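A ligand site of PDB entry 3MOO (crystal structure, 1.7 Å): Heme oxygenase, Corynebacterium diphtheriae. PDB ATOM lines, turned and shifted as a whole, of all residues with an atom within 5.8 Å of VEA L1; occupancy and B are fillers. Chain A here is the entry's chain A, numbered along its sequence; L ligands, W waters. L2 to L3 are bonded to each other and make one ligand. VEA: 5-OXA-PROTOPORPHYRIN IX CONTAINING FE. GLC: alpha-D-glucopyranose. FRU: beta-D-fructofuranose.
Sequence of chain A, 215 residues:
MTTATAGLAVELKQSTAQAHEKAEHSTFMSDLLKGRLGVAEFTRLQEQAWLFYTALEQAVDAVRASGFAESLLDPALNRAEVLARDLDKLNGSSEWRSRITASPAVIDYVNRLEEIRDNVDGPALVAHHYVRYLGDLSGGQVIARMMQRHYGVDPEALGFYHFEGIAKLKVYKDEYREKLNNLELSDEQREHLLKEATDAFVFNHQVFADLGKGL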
ATOM      1  N   ALA A   9       5.843 -15.435  17.998  1.00  0.00           N
ATOM      2  CA  ALA A   9       5.931 -14.425  19.073  1.00  0.00           C
ATOM      3  C   ALA A   9       7.095 -13.461  18.820  1.00  0.00           C
ATOM      4  O   ALA A   9       6.920 -12.231  18.937  1.00  0.00           O
ATOM      5  CB  ALA A   9       6.033 -15.068  20.459  1.00  0.00           C
ATOM      6  N   LEU A  12       6.456 -11.237  15.663  1.00  0.00           N
ATOM      7  CA  LEU A  12       5.482 -10.200  16.004  1.00  0.00           C
ATOM      8  C   LEU A  12       6.169  -9.037  16.721  1.00  0.00           C
ATOM      9  O   LEU A  12       5.976  -7.859  16.370  1.00  0.00           O
ATOM     10  CB  LEU A  12       4.421 -10.806  16.902  1.00  0.00           C
ATOM     11  CG  LEU A  12       2.940 -10.465  16.843  1.00  0.00           C
ATOM     12  CD1 LEU A  12       2.433  -9.911  15.480  1.00  0.00           C
ATOM     13  CD2 LEU A  12       2.161 -11.699  17.299  1.00  0.00           C
ATOM     14  N   LYS A  13       6.982  -9.363  17.719  1.00  0.00           N
ATOM     15  CA  LYS A  13       7.687  -8.329  18.496  1.00  0.00           C
ATOM     16  C   LYS A  13       8.623  -7.527  17.591  1.00  0.00           C
ATOM     17  O   LYS A  13       8.684  -6.292  17.676  1.00  0.00           O
ATOM     18  CB  LYS A  13       8.479  -8.970  19.639  1.00  0.00           C
ATOM     19  CG  LYS A  13       9.076  -7.993  20.654  1.00  0.00           C
ATOM     20  CD  LYS A  13       9.793  -8.807  21.756  1.00  0.00           C
ATOM     21  CE  LYS A  13      10.281  -7.957  22.931  1.00  0.00           C
ATOM     22  NZ  LYS A  13      11.296  -6.972  22.496  1.00  0.00           N
ATOM     23  N   HIS A  20       5.781   0.249  17.881  1.00  0.00           N
ATOM     24  CA  HIS A  20       5.783   0.385  19.346  1.00  0.00           C
ATOM     25  C   HIS A  20       6.501   1.641  19.812  1.00  0.00           C
ATOM     26  O   HIS A  20       5.996   2.384  20.639  1.00  0.00           O
ATOM     27  CB  HIS A  20       6.411  -0.830  20.049  1.00  0.00           C
ATOM     28  CG  HIS A  20       6.333  -0.747  21.540  1.00  0.00           C
ATOM     29  ND1 HIS A  20       7.272  -0.108  22.314  1.00  0.00           N
ATOM     30  CD2 HIS A  20       5.393  -1.216  22.395  1.00  0.00           C
ATOM     31  CE1 HIS A  20       6.925  -0.176  23.594  1.00  0.00           C
ATOM     32  NE2 HIS A  20       5.782  -0.841  23.674  1.00  0.00           N
ATOM     33  N   ALA A  23       4.485   4.675  19.047  1.00  0.00           N
ATOM     34  CA  ALA A  23       3.324   4.743  19.969  1.00  0.00           C
ATOM     35  C   ALA A  23       3.736   5.321  21.311  1.00  0.00           C
ATOM     36  O   ALA A  23       3.073   6.206  21.863  1.00  0.00           O
ATOM     37  CB  ALA A  23       2.715   3.331  20.181  1.00  0.00           C
ATOM     38  N   GLU A  24       4.855   4.805  21.806  1.00  0.00           N
ATOM     39  CA  GLU A  24       5.403   5.155  23.088  1.00  0.00           C
ATOM     40  C   GLU A  24       5.828   6.630  23.134  1.00  0.00           C
ATOM     41  O   GLU A  24       5.699   7.260  24.171  1.00  0.00           O
ATOM     42  CB  GLU A  24       6.584   4.212  23.403  1.00  0.00           C
ATOM     43  CG  GLU A  24       7.287   4.460  24.724  1.00  0.00           C
ATOM     44  CD  GLU A  24       8.521   3.621  24.867  1.00  0.00           C
ATOM     45  OE1 GLU A  24       9.628   4.187  24.883  1.00  0.00           O
ATOM     46  OE2 GLU A  24       8.386   2.385  24.924  1.00  0.00           O
ATOM     47  N   HIS A  25       6.261   7.165  21.989  1.00  0.00           N
ATOM     48  CA  HIS A  25       6.760   8.556  21.911  1.00  0.00           C
ATOM     49  C   HIS A  25       5.796   9.604  21.301  1.00  0.00           C
ATOM     50  O   HIS A  25       6.176  10.749  21.059  1.00  0.00           O
ATOM     51  CB  HIS A  25       8.130   8.601  21.216  1.00  0.00           C
ATOM     52  CG  HIS A  25       9.192   7.826  21.919  1.00  0.00           C
ATOM     53  ND1 HIS A  25       9.719   8.212  23.136  1.00  0.00           N
ATOM     54  CD2 HIS A  25       9.809   6.671  21.592  1.00  0.00           C
ATOM     55  CE1 HIS A  25      10.625   7.331  23.514  1.00  0.00           C
ATOM     56  NE2 HIS A  25      10.695   6.386  22.605  1.00  0.00           N
ATOM     57  N   MET A  29       0.849  10.728  24.805  1.00  0.00           N
ATOM     58  CA  MET A  29       1.229   9.664  25.749  1.00  0.00           C
ATOM     59  C   MET A  29       2.495  10.045  26.515  1.00  0.00           C
ATOM     60  O   MET A  29       2.595   9.826  27.732  1.00  0.00           O
ATOM     61  CB  MET A  29       1.376   8.321  25.025  1.00  0.00           C
ATOM     62  CG  MET A  29       1.561   7.104  25.936  1.00  0.00           C
ATOM     63  SD  MET A  29       0.465   7.055  27.379  1.00  0.00           S
ATOM     64  CE  MET A  29      -1.116   7.261  26.552  1.00  0.00           C
ATOM     65  N   SER A  30       3.451  10.656  25.804  1.00  0.00           N
ATOM     66  CA  SER A  30       4.678  11.166  26.375  1.00  0.00           C
ATOM     67  C   SER A  30       4.392  12.186  27.484  1.00  0.00           C
ATOM     68  O   SER A  30       4.882  12.050  28.616  1.00  0.00           O
ATOM     69  CB  SER A  30       5.566  11.775  25.276  1.00  0.00           C
ATOM     70  OG  SER A  30       6.789  12.225  25.819  1.00  0.00           O
ATOM     71  N   LEU A  33       2.506  10.516  30.573  1.00  0.00           N
ATOM     72  CA  LEU A  33       3.344   9.682  31.436  1.00  0.00           C
ATOM     73  C   LEU A  33       4.411  10.454  32.192  1.00  0.00           C
ATOM     74  O   LEU A  33       4.845  10.034  33.278  1.00  0.00           O
ATOM     75  CB  LEU A  33       3.987   8.558  30.612  1.00  0.00           C
ATOM     76  CG  LEU A  33       2.996   7.480  30.205  1.00  0.00           C
ATOM     77  CD1 LEU A  33       3.682   6.385  29.397  1.00  0.00           C
ATOM     78  CD2 LEU A  33       2.353   6.876  31.449  1.00  0.00           C
ATOM     79  N   TYR A 130      -3.217  -9.200  20.802  1.00  0.00           N
ATOM     80  CA  TYR A 130      -1.806  -9.095  21.236  1.00  0.00           C
ATOM     81  C   TYR A 130      -1.420  -7.631  21.499  1.00  0.00           C
ATOM     82  O   TYR A 130      -0.855  -7.309  22.552  1.00  0.00           O
ATOM     83  CB  TYR A 130      -0.911  -9.703  20.154  1.00  0.00           C
ATOM     84  CG  TYR A 130       0.521  -9.243  20.194  1.00  0.00           C
ATOM     85  CD1 TYR A 130       1.441  -9.808  21.131  1.00  0.00           C
ATOM     86  CD2 TYR A 130       1.002  -8.288  19.299  1.00  0.00           C
ATOM     87  CE1 TYR A 130       2.771  -9.431  21.128  1.00  0.00           C
ATOM     88  CE2 TYR A 130       2.347  -7.887  19.305  1.00  0.00           C
ATOM     89  CZ  TYR A 130       3.222  -8.450  20.254  1.00  0.00           C
ATOM     90  OH  TYR A 130       4.544  -8.068  20.241  1.00  0.00           O
ATOM     91  N   VAL A 131      -1.752  -6.739  20.566  1.00  0.00           N
ATOM     92  CA  VAL A 131      -1.274  -5.356  20.628  1.00  0.00           C
ATOM     93  C   VAL A 131      -1.860  -4.652  21.874  1.00  0.00           C
ATOM     94  O   VAL A 131      -1.133  -3.984  22.604  1.00  0.00           O
ATOM     95  CB  VAL A 131      -1.565  -4.564  19.323  1.00  0.00           C
ATOM     96  CG1 VAL A 131      -1.353  -3.062  19.500  1.00  0.00           C
ATOM     97  CG2 VAL A 131      -0.684  -5.071  18.184  1.00  0.00           C
ATOM     98  N   ARG A 132      -3.153  -4.833  22.112  1.00  0.00           N
ATOM     99  CA  ARG A 132      -3.803  -4.202  23.287  1.00  0.00           C
ATOM    100  C   ARG A 132      -3.462  -4.922  24.594  1.00  0.00           C
ATOM    101  O   ARG A 132      -2.886  -4.333  25.539  1.00  0.00           O
ATOM    102  CB  ARG A 132      -5.324  -4.076  23.110  1.00  0.00           C
ATOM    103  CG  ARG A 132      -5.776  -2.915  22.182  1.00  0.00           C
ATOM    104  CD  ARG A 132      -5.114  -1.539  22.536  1.00  0.00           C
ATOM    105  NE  ARG A 132      -5.123  -1.248  23.978  1.00  0.00           N
ATOM    106  CZ  ARG A 132      -4.678  -0.147  24.567  1.00  0.00           C
ATOM    107  NH1 ARG A 132      -4.164   0.849  23.860  1.00  0.00           N
ATOM    108  NH2 ARG A 132      -4.736  -0.029  25.901  1.00  0.00           N
ATOM    109  N   LEU A 134      -1.317  -7.427  25.538  1.00  0.00           N
ATOM    110  CA  LEU A 134       0.085  -7.530  25.984  1.00  0.00           C
ATOM    111  C   LEU A 134       0.661  -6.153  26.346  1.00  0.00           C
ATOM    112  O   LEU A 134       1.468  -6.053  27.284  1.00  0.00           O
ATOM    113  CB  LEU A 134       0.963  -8.319  25.021  1.00  0.00           C
ATOM    114  CG  LEU A 134       1.261  -9.728  25.537  1.00  0.00           C
ATOM    115  CD1 LEU A 134      -0.039 -10.516  25.533  1.00  0.00           C
ATOM    116  CD2 LEU A 134       2.362 -10.395  24.688  1.00  0.00           C
ATOM    117  N   GLY A 135       0.170  -5.092  25.704  1.00  0.00           N
ATOM    118  CA  GLY A 135       0.462  -3.724  26.130  1.00  0.00           C
ATOM    119  C   GLY A 135      -0.018  -3.464  27.563  1.00  0.00           C
ATOM    120  O   GLY A 135       0.755  -2.982  28.412  1.00  0.00           O
ATOM    121  N   LEU A 137      -0.669  -5.553  29.987  1.00  0.00           N
ATOM    122  CA  LEU A 137       0.158  -6.402  30.861  1.00  0.00           C
ATOM    123  C   LEU A 137       1.618  -5.984  30.946  1.00  0.00           C
ATOM    124  O   LEU A 137       2.393  -6.555  31.704  1.00  0.00           O
ATOM    125  CB  LEU A 137       0.094  -7.826  30.346  1.00  0.00           C
ATOM    126  CG  LEU A 137      -1.319  -8.412  30.410  1.00  0.00           C
ATOM    127  CD1 LEU A 137      -1.430  -9.629  29.497  1.00  0.00           C
ATOM    128  CD2 LEU A 137      -1.723  -8.765  31.832  1.00  0.00           C
ATOM    129  N   SER A 138       1.990  -4.933  30.225  1.00  0.00           N
ATOM    130  CA  SER A 138       3.392  -4.548  30.086  1.00  0.00           C
ATOM    131  C   SER A 138       3.534  -3.109  30.525  1.00  0.00           C
ATOM    132  O   SER A 138       3.488  -2.841  31.740  1.00  0.00           O
ATOM    133  CB  SER A 138       3.871  -4.788  28.644  1.00  0.00           C
ATOM    134  OG  SER A 138       3.946  -6.181  28.357  1.00  0.00           O
ATOM    135  N   GLY A 139       3.671  -2.190  29.571  1.00  0.00           N
ATOM    136  CA  GLY A 139       3.744  -0.752  29.855  1.00  0.00           C
ATOM    137  C   GLY A 139       2.525  -0.232  30.601  1.00  0.00           C
ATOM    138  O   GLY A 139       2.625   0.755  31.331  1.00  0.00           O
ATOM    139  N   VAL A 142       3.181   0.319  34.198  1.00  0.00           N
ATOM    140  CA  VAL A 142       3.899   1.587  34.432  1.00  0.00           C
ATOM    141  C   VAL A 142       2.920   2.766  34.374  1.00  0.00           C
ATOM    142  O   VAL A 142       2.955   3.673  35.215  1.00  0.00           O
ATOM    143  CB  VAL A 142       5.047   1.766  33.382  1.00  0.00           C
ATOM    144  CG1 VAL A 142       5.702   3.144  33.494  1.00  0.00           C
ATOM    145  CG2 VAL A 142       6.089   0.622  33.504  1.00  0.00           C
ATOM    146  N   ILE A 143       2.058   2.769  33.376  1.00  0.00           N
ATOM    147  CA  ILE A 143       1.037   3.807  33.241  1.00  0.00           C
ATOM    148  C   ILE A 143       0.227   3.948  34.527  1.00  0.00           C
ATOM    149  O   ILE A 143       0.049   5.061  35.011  1.00  0.00           O
ATOM    150  CB  ILE A 143       0.121   3.563  32.029  1.00  0.00           C
ATOM    151  CG1 ILE A 143       0.954   3.597  30.742  1.00  0.00           C
ATOM    152  CG2 ILE A 143      -1.054   4.581  32.040  1.00  0.00           C
ATOM    153  CD1 ILE A 143       0.178   3.253  29.450  1.00  0.00           C
ATOM    154  N   LYS A 173       2.437 -13.790  30.379  1.00  0.00           N
ATOM    155  CA  LYS A 173       2.906 -13.362  29.072  1.00  0.00           C
ATOM    156  C   LYS A 173       3.731 -14.441  28.369  1.00  0.00           C
ATOM    157  O   LYS A 173       3.583 -14.631  27.170  1.00  0.00           O
ATOM    158  CB  LYS A 173       3.619 -12.011  29.177  1.00  0.00           C
ATOM    159  CG  LYS A 173       2.660 -10.919  29.636  1.00  0.00           C
ATOM    160  CD  LYS A 173       3.356  -9.940  30.580  1.00  0.00           C
ATOM    161  CE  LYS A 173       4.033  -8.854  29.778  1.00  0.00           C
ATOM    162  NZ  LYS A 173       5.310  -8.316  30.338  1.00  0.00           N
ATOM    163  N   ARG A 177       2.806 -16.044  24.783  1.00  0.00           N
ATOM    164  CA  ARG A 177       3.731 -16.163  23.661  1.00  0.00           C
ATOM    165  C   ARG A 177       3.834 -17.605  23.157  1.00  0.00           C
ATOM    166  O   ARG A 177       3.904 -17.847  21.953  1.00  0.00           O
ATOM    167  CB  ARG A 177       5.100 -15.596  24.024  1.00  0.00           C
ATOM    168  CG  ARG A 177       5.133 -14.089  24.166  1.00  0.00           C
ATOM    169  CD  ARG A 177       6.544 -13.582  24.395  1.00  0.00           C
ATOM    170  NE  ARG A 177       6.482 -12.236  24.884  1.00  0.00           N
ATOM    171  CZ  ARG A 177       6.446 -11.895  26.179  1.00  0.00           C
ATOM    172  NH1 ARG A 177       6.517 -12.805  27.131  1.00  0.00           N
ATOM    173  NH2 ARG A 177       6.344 -10.602  26.522  1.00  0.00           N
ATOM    174  N   ALA A 200      -2.747  -2.255  13.954  1.00  0.00           N
ATOM    175  CA  ALA A 200      -3.285  -2.058  15.324  1.00  0.00           C
ATOM    176  C   ALA A 200      -2.481  -0.975  16.087  1.00  0.00           C
ATOM    177  O   ALA A 200      -3.055  -0.069  16.731  1.00  0.00           O
ATOM    178  CB  ALA A 200      -3.283  -3.415  16.095  1.00  0.00           C
ATOM    179  N   PHE A 201      -1.157  -1.050  15.997  1.00  0.00           N
ATOM    180  CA  PHE A 201      -0.298  -0.020  16.607  1.00  0.00           C
ATOM    181  C   PHE A 201      -0.593   1.338  15.978  1.00  0.00           C
ATOM    182  O   PHE A 201      -0.639   2.358  16.686  1.00  0.00           O
ATOM    183  CB  PHE A 201       1.178  -0.366  16.417  1.00  0.00           C
ATOM    184  CG  PHE A 201       1.753  -1.171  17.543  1.00  0.00           C
ATOM    185  CD1 PHE A 201       2.028  -0.578  18.794  1.00  0.00           C
ATOM    186  CD2 PHE A 201       2.004  -2.529  17.369  1.00  0.00           C
ATOM    187  CE1 PHE A 201       2.577  -1.350  19.826  1.00  0.00           C
ATOM    188  CE2 PHE A 201       2.537  -3.306  18.383  1.00  0.00           C
ATOM    189  CZ  PHE A 201       2.795  -2.730  19.630  1.00  0.00           C
ATOM    190  N   ASN A 204      -3.717   2.935  17.329  1.00  0.00           N
ATOM    191  CA  ASN A 204      -3.435   3.506  18.656  1.00  0.00           C
ATOM    192  C   ASN A 204      -2.653   4.819  18.582  1.00  0.00           C
ATOM    193  O   ASN A 204      -2.975   5.770  19.314  1.00  0.00           O
ATOM    194  CB  ASN A 204      -2.735   2.474  19.543  1.00  0.00           C
ATOM    195  CG  ASN A 204      -3.711   1.421  20.041  1.00  0.00           C
ATOM    196  OD1 ASN A 204      -3.936   0.385  19.393  1.00  0.00           O
ATOM    197  ND2 ASN A 204      -4.369   1.722  21.132  1.00  0.00           N
ATOM    198  N   PHE A 208      -3.988   8.492  20.021  1.00  0.00           N
ATOM    199  CA  PHE A 208      -3.225   9.426  20.888  1.00  0.00           C
ATOM    200  C   PHE A 208      -3.140  10.804  20.225  1.00  0.00           C
ATOM    201  O   PHE A 208      -3.200  11.813  20.908  1.00  0.00           O
ATOM    202  CB  PHE A 208      -1.815   8.930  21.234  1.00  0.00           C
ATOM    203  CG  PHE A 208      -1.784   7.579  21.916  1.00  0.00           C
ATOM    204  CD1 PHE A 208      -2.794   7.203  22.825  1.00  0.00           C
ATOM    205  CD2 PHE A 208      -0.736   6.697  21.681  1.00  0.00           C
ATOM    206  CE1 PHE A 208      -2.764   5.947  23.445  1.00  0.00           C
ATOM    207  CE2 PHE A 208      -0.694   5.443  22.290  1.00  0.00           C
ATOM    208  CZ  PHE A 208      -1.709   5.071  23.175  1.00  0.00           C
HETATM  209  O2D VEA L   1       5.998  -9.056  22.107  1.00  0.00           O
HETATM  210  CGD VEA L   1       6.307  -8.458  23.162  1.00  0.00           C
HETATM  211  O1D VEA L   1       6.830  -9.039  24.122  1.00  0.00           O
HETATM  212  CBD VEA L   1       6.027  -6.979  23.281  1.00  0.00           C
HETATM  213  CAD VEA L   1       4.812  -6.820  24.186  1.00  0.00           C
HETATM  214  C3D VEA L   1       4.299  -5.389  24.136  1.00  0.00           C
HETATM  215  C2D VEA L   1       3.210  -4.928  23.416  1.00  0.00           C
HETATM  216  C5D VEA L   1       2.235  -5.600  22.460  1.00  0.00           C
HETATM  217  C4D VEA L   1       4.838  -4.241  24.869  1.00  0.00           C
HETATM  218  CHA VEA L   1       5.952  -4.250  25.730  1.00  0.00           C
HETATM  219  N1  VEA L   1       4.188  -3.041  24.409  1.00  0.00           N
HETATM  220  C1D VEA L   1       3.063  -3.483  23.663  1.00  0.00           C
HETATM  221  CHD VEA L   1       2.146  -2.597  23.194  1.00  0.00           C
HETATM  222  C4C VEA L   1       2.095  -1.249  23.497  1.00  0.00           C
HETATM  223  C3C VEA L   1       1.102  -0.338  22.936  1.00  0.00           C
HETATM  224  CAC VEA L   1       0.047  -0.833  22.013  1.00  0.00           C
HETATM  225  CBC VEA L   1      -1.107  -0.185  21.933  1.00  0.00           C
HETATM  226  C2C VEA L   1       1.296   0.915  23.373  1.00  0.00           C
HETATM  227  C5C VEA L   1       0.573   2.228  23.145  1.00  0.00           C
HETATM  228 FE   VEA L   1       4.510  -1.333  25.310  1.00  0.00          FE
HETATM  229  N2  VEA L   1       6.026  -1.877  26.446  1.00  0.00           N
HETATM  230  C1A VEA L   1       6.497  -3.154  26.430  1.00  0.00           C
HETATM  231  N3  VEA L   1       2.878  -0.569  24.378  1.00  0.00           N
HETATM  232  C1C VEA L   1       2.448   0.685  24.186  1.00  0.00           C
HETATM  233  O   VEA L   1       2.849   1.788  24.786  1.00  0.00           O
HETATM  234  C4B VEA L   1       3.810   1.725  25.628  1.00  0.00           C
HETATM  235  C3B VEA L   1       4.360   2.885  26.305  1.00  0.00           C
HETATM  236  CAB VEA L   1       3.827   4.265  26.287  1.00  0.00           C
HETATM  237  CBB VEA L   1       4.616   5.293  26.525  1.00  0.00           C
HETATM  238  C2B VEA L   1       5.373   2.390  27.015  1.00  0.00           C
HETATM  239  C5B VEA L   1       6.413   2.986  27.974  1.00  0.00           C
HETATM  240  N4  VEA L   1       4.497   0.625  25.628  1.00  0.00           N
HETATM  241  C1B VEA L   1       5.428   0.966  26.658  1.00  0.00           C
HETATM  242  CHB VEA L   1       6.477   0.255  27.282  1.00  0.00           C
HETATM  243  C4A VEA L   1       6.789  -1.088  27.195  1.00  0.00           C
HETATM  244  C3A VEA L   1       7.823  -1.968  27.786  1.00  0.00           C
HETATM  245  C5A VEA L   1       8.856  -1.409  28.752  1.00  0.00           C
HETATM  246  C2A VEA L   1       7.633  -3.236  27.336  1.00  0.00           C
HETATM  247  CAA VEA L   1       8.475  -4.490  27.640  1.00  0.00           C
HETATM  248  CBA VEA L   1       7.722  -5.481  28.523  1.00  0.00           C
HETATM  249  CGA VEA L   1       7.514  -4.930  29.915  1.00  0.00           C
HETATM  250  O1A VEA L   1       6.543  -5.325  30.579  1.00  0.00           O
HETATM  251  O2A VEA L   1       8.325  -4.090  30.375  1.00  0.00           O
HETATM  252  C1  GLC L   2      13.322  -0.604  22.526  1.00  0.00           C
HETATM  253  C2  GLC L   2      14.800  -0.475  22.160  1.00  0.00           C
HETATM  254  C3  GLC L   2      15.559  -1.641  22.754  1.00  0.00           C
HETATM  255  C4  GLC L   2      15.319  -1.733  24.264  1.00  0.00           C
HETATM  256  C5  GLC L   2      13.822  -1.783  24.564  1.00  0.00           C
HETATM  257  C6  GLC L   2      13.540  -1.803  26.069  1.00  0.00           C
HETATM  258  O2  GLC L   2      14.929  -0.459  20.735  1.00  0.00           O
HETATM  259  O3  GLC L   2      16.961  -1.483  22.557  1.00  0.00           O
HETATM  260  O4  GLC L   2      16.021  -2.875  24.727  1.00  0.00           O
HETATM  261  O5  GLC L   2      13.221  -0.621  23.964  1.00  0.00           O
HETATM  262  O6  GLC L   2      12.145  -1.621  26.385  1.00  0.00           O
HETATM  263  C1  FRU L   3      11.271  -0.665  20.419  1.00  0.00           C
HETATM  264  C2  FRU L   3      11.454  -1.757  21.470  1.00  0.00           C
HETATM  265  C3  FRU L   3      11.090  -3.125  20.903  1.00  0.00           C
HETATM  266  C4  FRU L   3      10.557  -3.842  22.119  1.00  0.00           C
HETATM  267  C5  FRU L   3       9.771  -2.743  22.815  1.00  0.00           C
HETATM  268  C6  FRU L   3       9.518  -2.974  24.305  1.00  0.00           C
HETATM  269  O1  FRU L   3      10.508   0.387  21.006  1.00  0.00           O
HETATM  270  O2  FRU L   3      12.809  -1.808  21.946  1.00  0.00           O
HETATM  271  O3  FRU L   3      12.246  -3.783  20.351  1.00  0.00           O
HETATM  272  O4  FRU L   3       9.769  -4.999  21.792  1.00  0.00           O
HETATM  273  O5  FRU L   3      10.539  -1.552  22.576  1.00  0.00           O
HETATM  274  O6  FRU L   3      10.735  -3.370  24.958  1.00  0.00           O
HETATM  275  O   HOH W   1       8.304  -7.609  26.049  1.00  0.00           O
HETATM  276  O   HOH W   2       9.194 -10.558  24.558  1.00  0.00           O
HETATM  277  O   HOH W   3       6.697 -11.609  21.734  1.00  0.00           O
HETATM  278  O   HOH W   4      -1.901  -1.780  24.836  1.00  0.00           O
HETATM  279  O   HOH W   5       5.393  -4.346  32.939  1.00  0.00           O
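FE of VEA L1 is bound by NE2 of His 20, at 2.1 Å. The side-chain amino group (NZ) of Lys 173 is in salt-bridge range of an oxygen (O1A) of VEA L1. An oxygen (O1D) of VEA L1 lies within salt-bridge range of the guanidinium group (NH2) of Arg 177, 2.9 Å away. O2D of VEA L1 sits at hydrogen-bond distance from OH of Tyr 130 (2.6 Å). NZ of Lys 13 lies within hydrogen-bond range of O4 of FRU L3 (2.6 Å).
The side-chain amino group (NZ) of Lys 173 sits close to the side-chain hydroxyl (OG) of Ser 138 (3.2 Å). OG of Ser 138 lies within hydrogen-bond range of O of Leu 134. OD1 of Asn 204 lies close to O of Ala 200, 2.8 Å away. NH1 of Arg 177 sits close to O of Lys 173, 3.5 Å away. OE1 of Glu 24 sits at hydrogen-bond distance from NE2 of His 25, 3.3 Å away. NH1 of Arg 132 sits close to ND2 of Asn 204 (2.9 Å).
Lys 13 touches VEA L1 (CB to O2D, 3.5 Å). Ala 23 touches VEA L1 (CB to C5C, 3.8 Å). O of Glu 24 touches CBB of VEA L1, at 3.3 Å. Met 29 touches VEA L1. Leu 33 touches VEA L1. O of Val 131 touches CAC of VEA L1, at 3.4 Å. NH1 of Arg 132 touches CBC of VEA L1, 3.8 Å away. Leu 134 touches VEA L1. Gly 135 touches VEA L1 (CA to CHD, 3.6 Å). CA of Ser 138 touches O1A of VEA L1, at 3.3 Å. Gly 139 touches VEA L1 (CA to CHB, 3.9 Å). Phe 201 touches VEA L1. Asn 204 touches VEA L1 (CG to CBC, 3.6 Å). CE2 of Phe 208 touches C5C of VEA L1, at 3.6 Å. Hydrophobic or aromatic side chains within 4 Å of VEA L1: His 20, Ala 23, Met 29, Leu 33, Tyr 130, Val 131, Leu 134, Phe 201 and Phe 208. Within 4 Å of VEA L1: Lys 13, His 20, Ala 23, Glu 24, Met 29, Leu 33, Tyr 130, Val 131, Arg 132, Leu 134, Gly 135, Ser 138, Gly 139, Lys 173, Arg 177, Phe 201, Asn 204 and Phe 208. The nearest printed residue that does not touch VEA L1 is Leu 137 (4.5 Å).
Water W3 lies within hydrogen-bond range of an oxygen (O2D) of VEA L1, the backbone carbonyl oxygen (O) of Ala 9 and the guanidinium group (NE) of Arg 177. Water W5 lies within hydrogen-bond range of O of Ser 138 (2.7 Å) and O1A of VEA L1 (2.8 Å). Water W2 bridges O1D of VEA L1 (2.8 Å) and NE of Arg 177 (3.2 Å).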
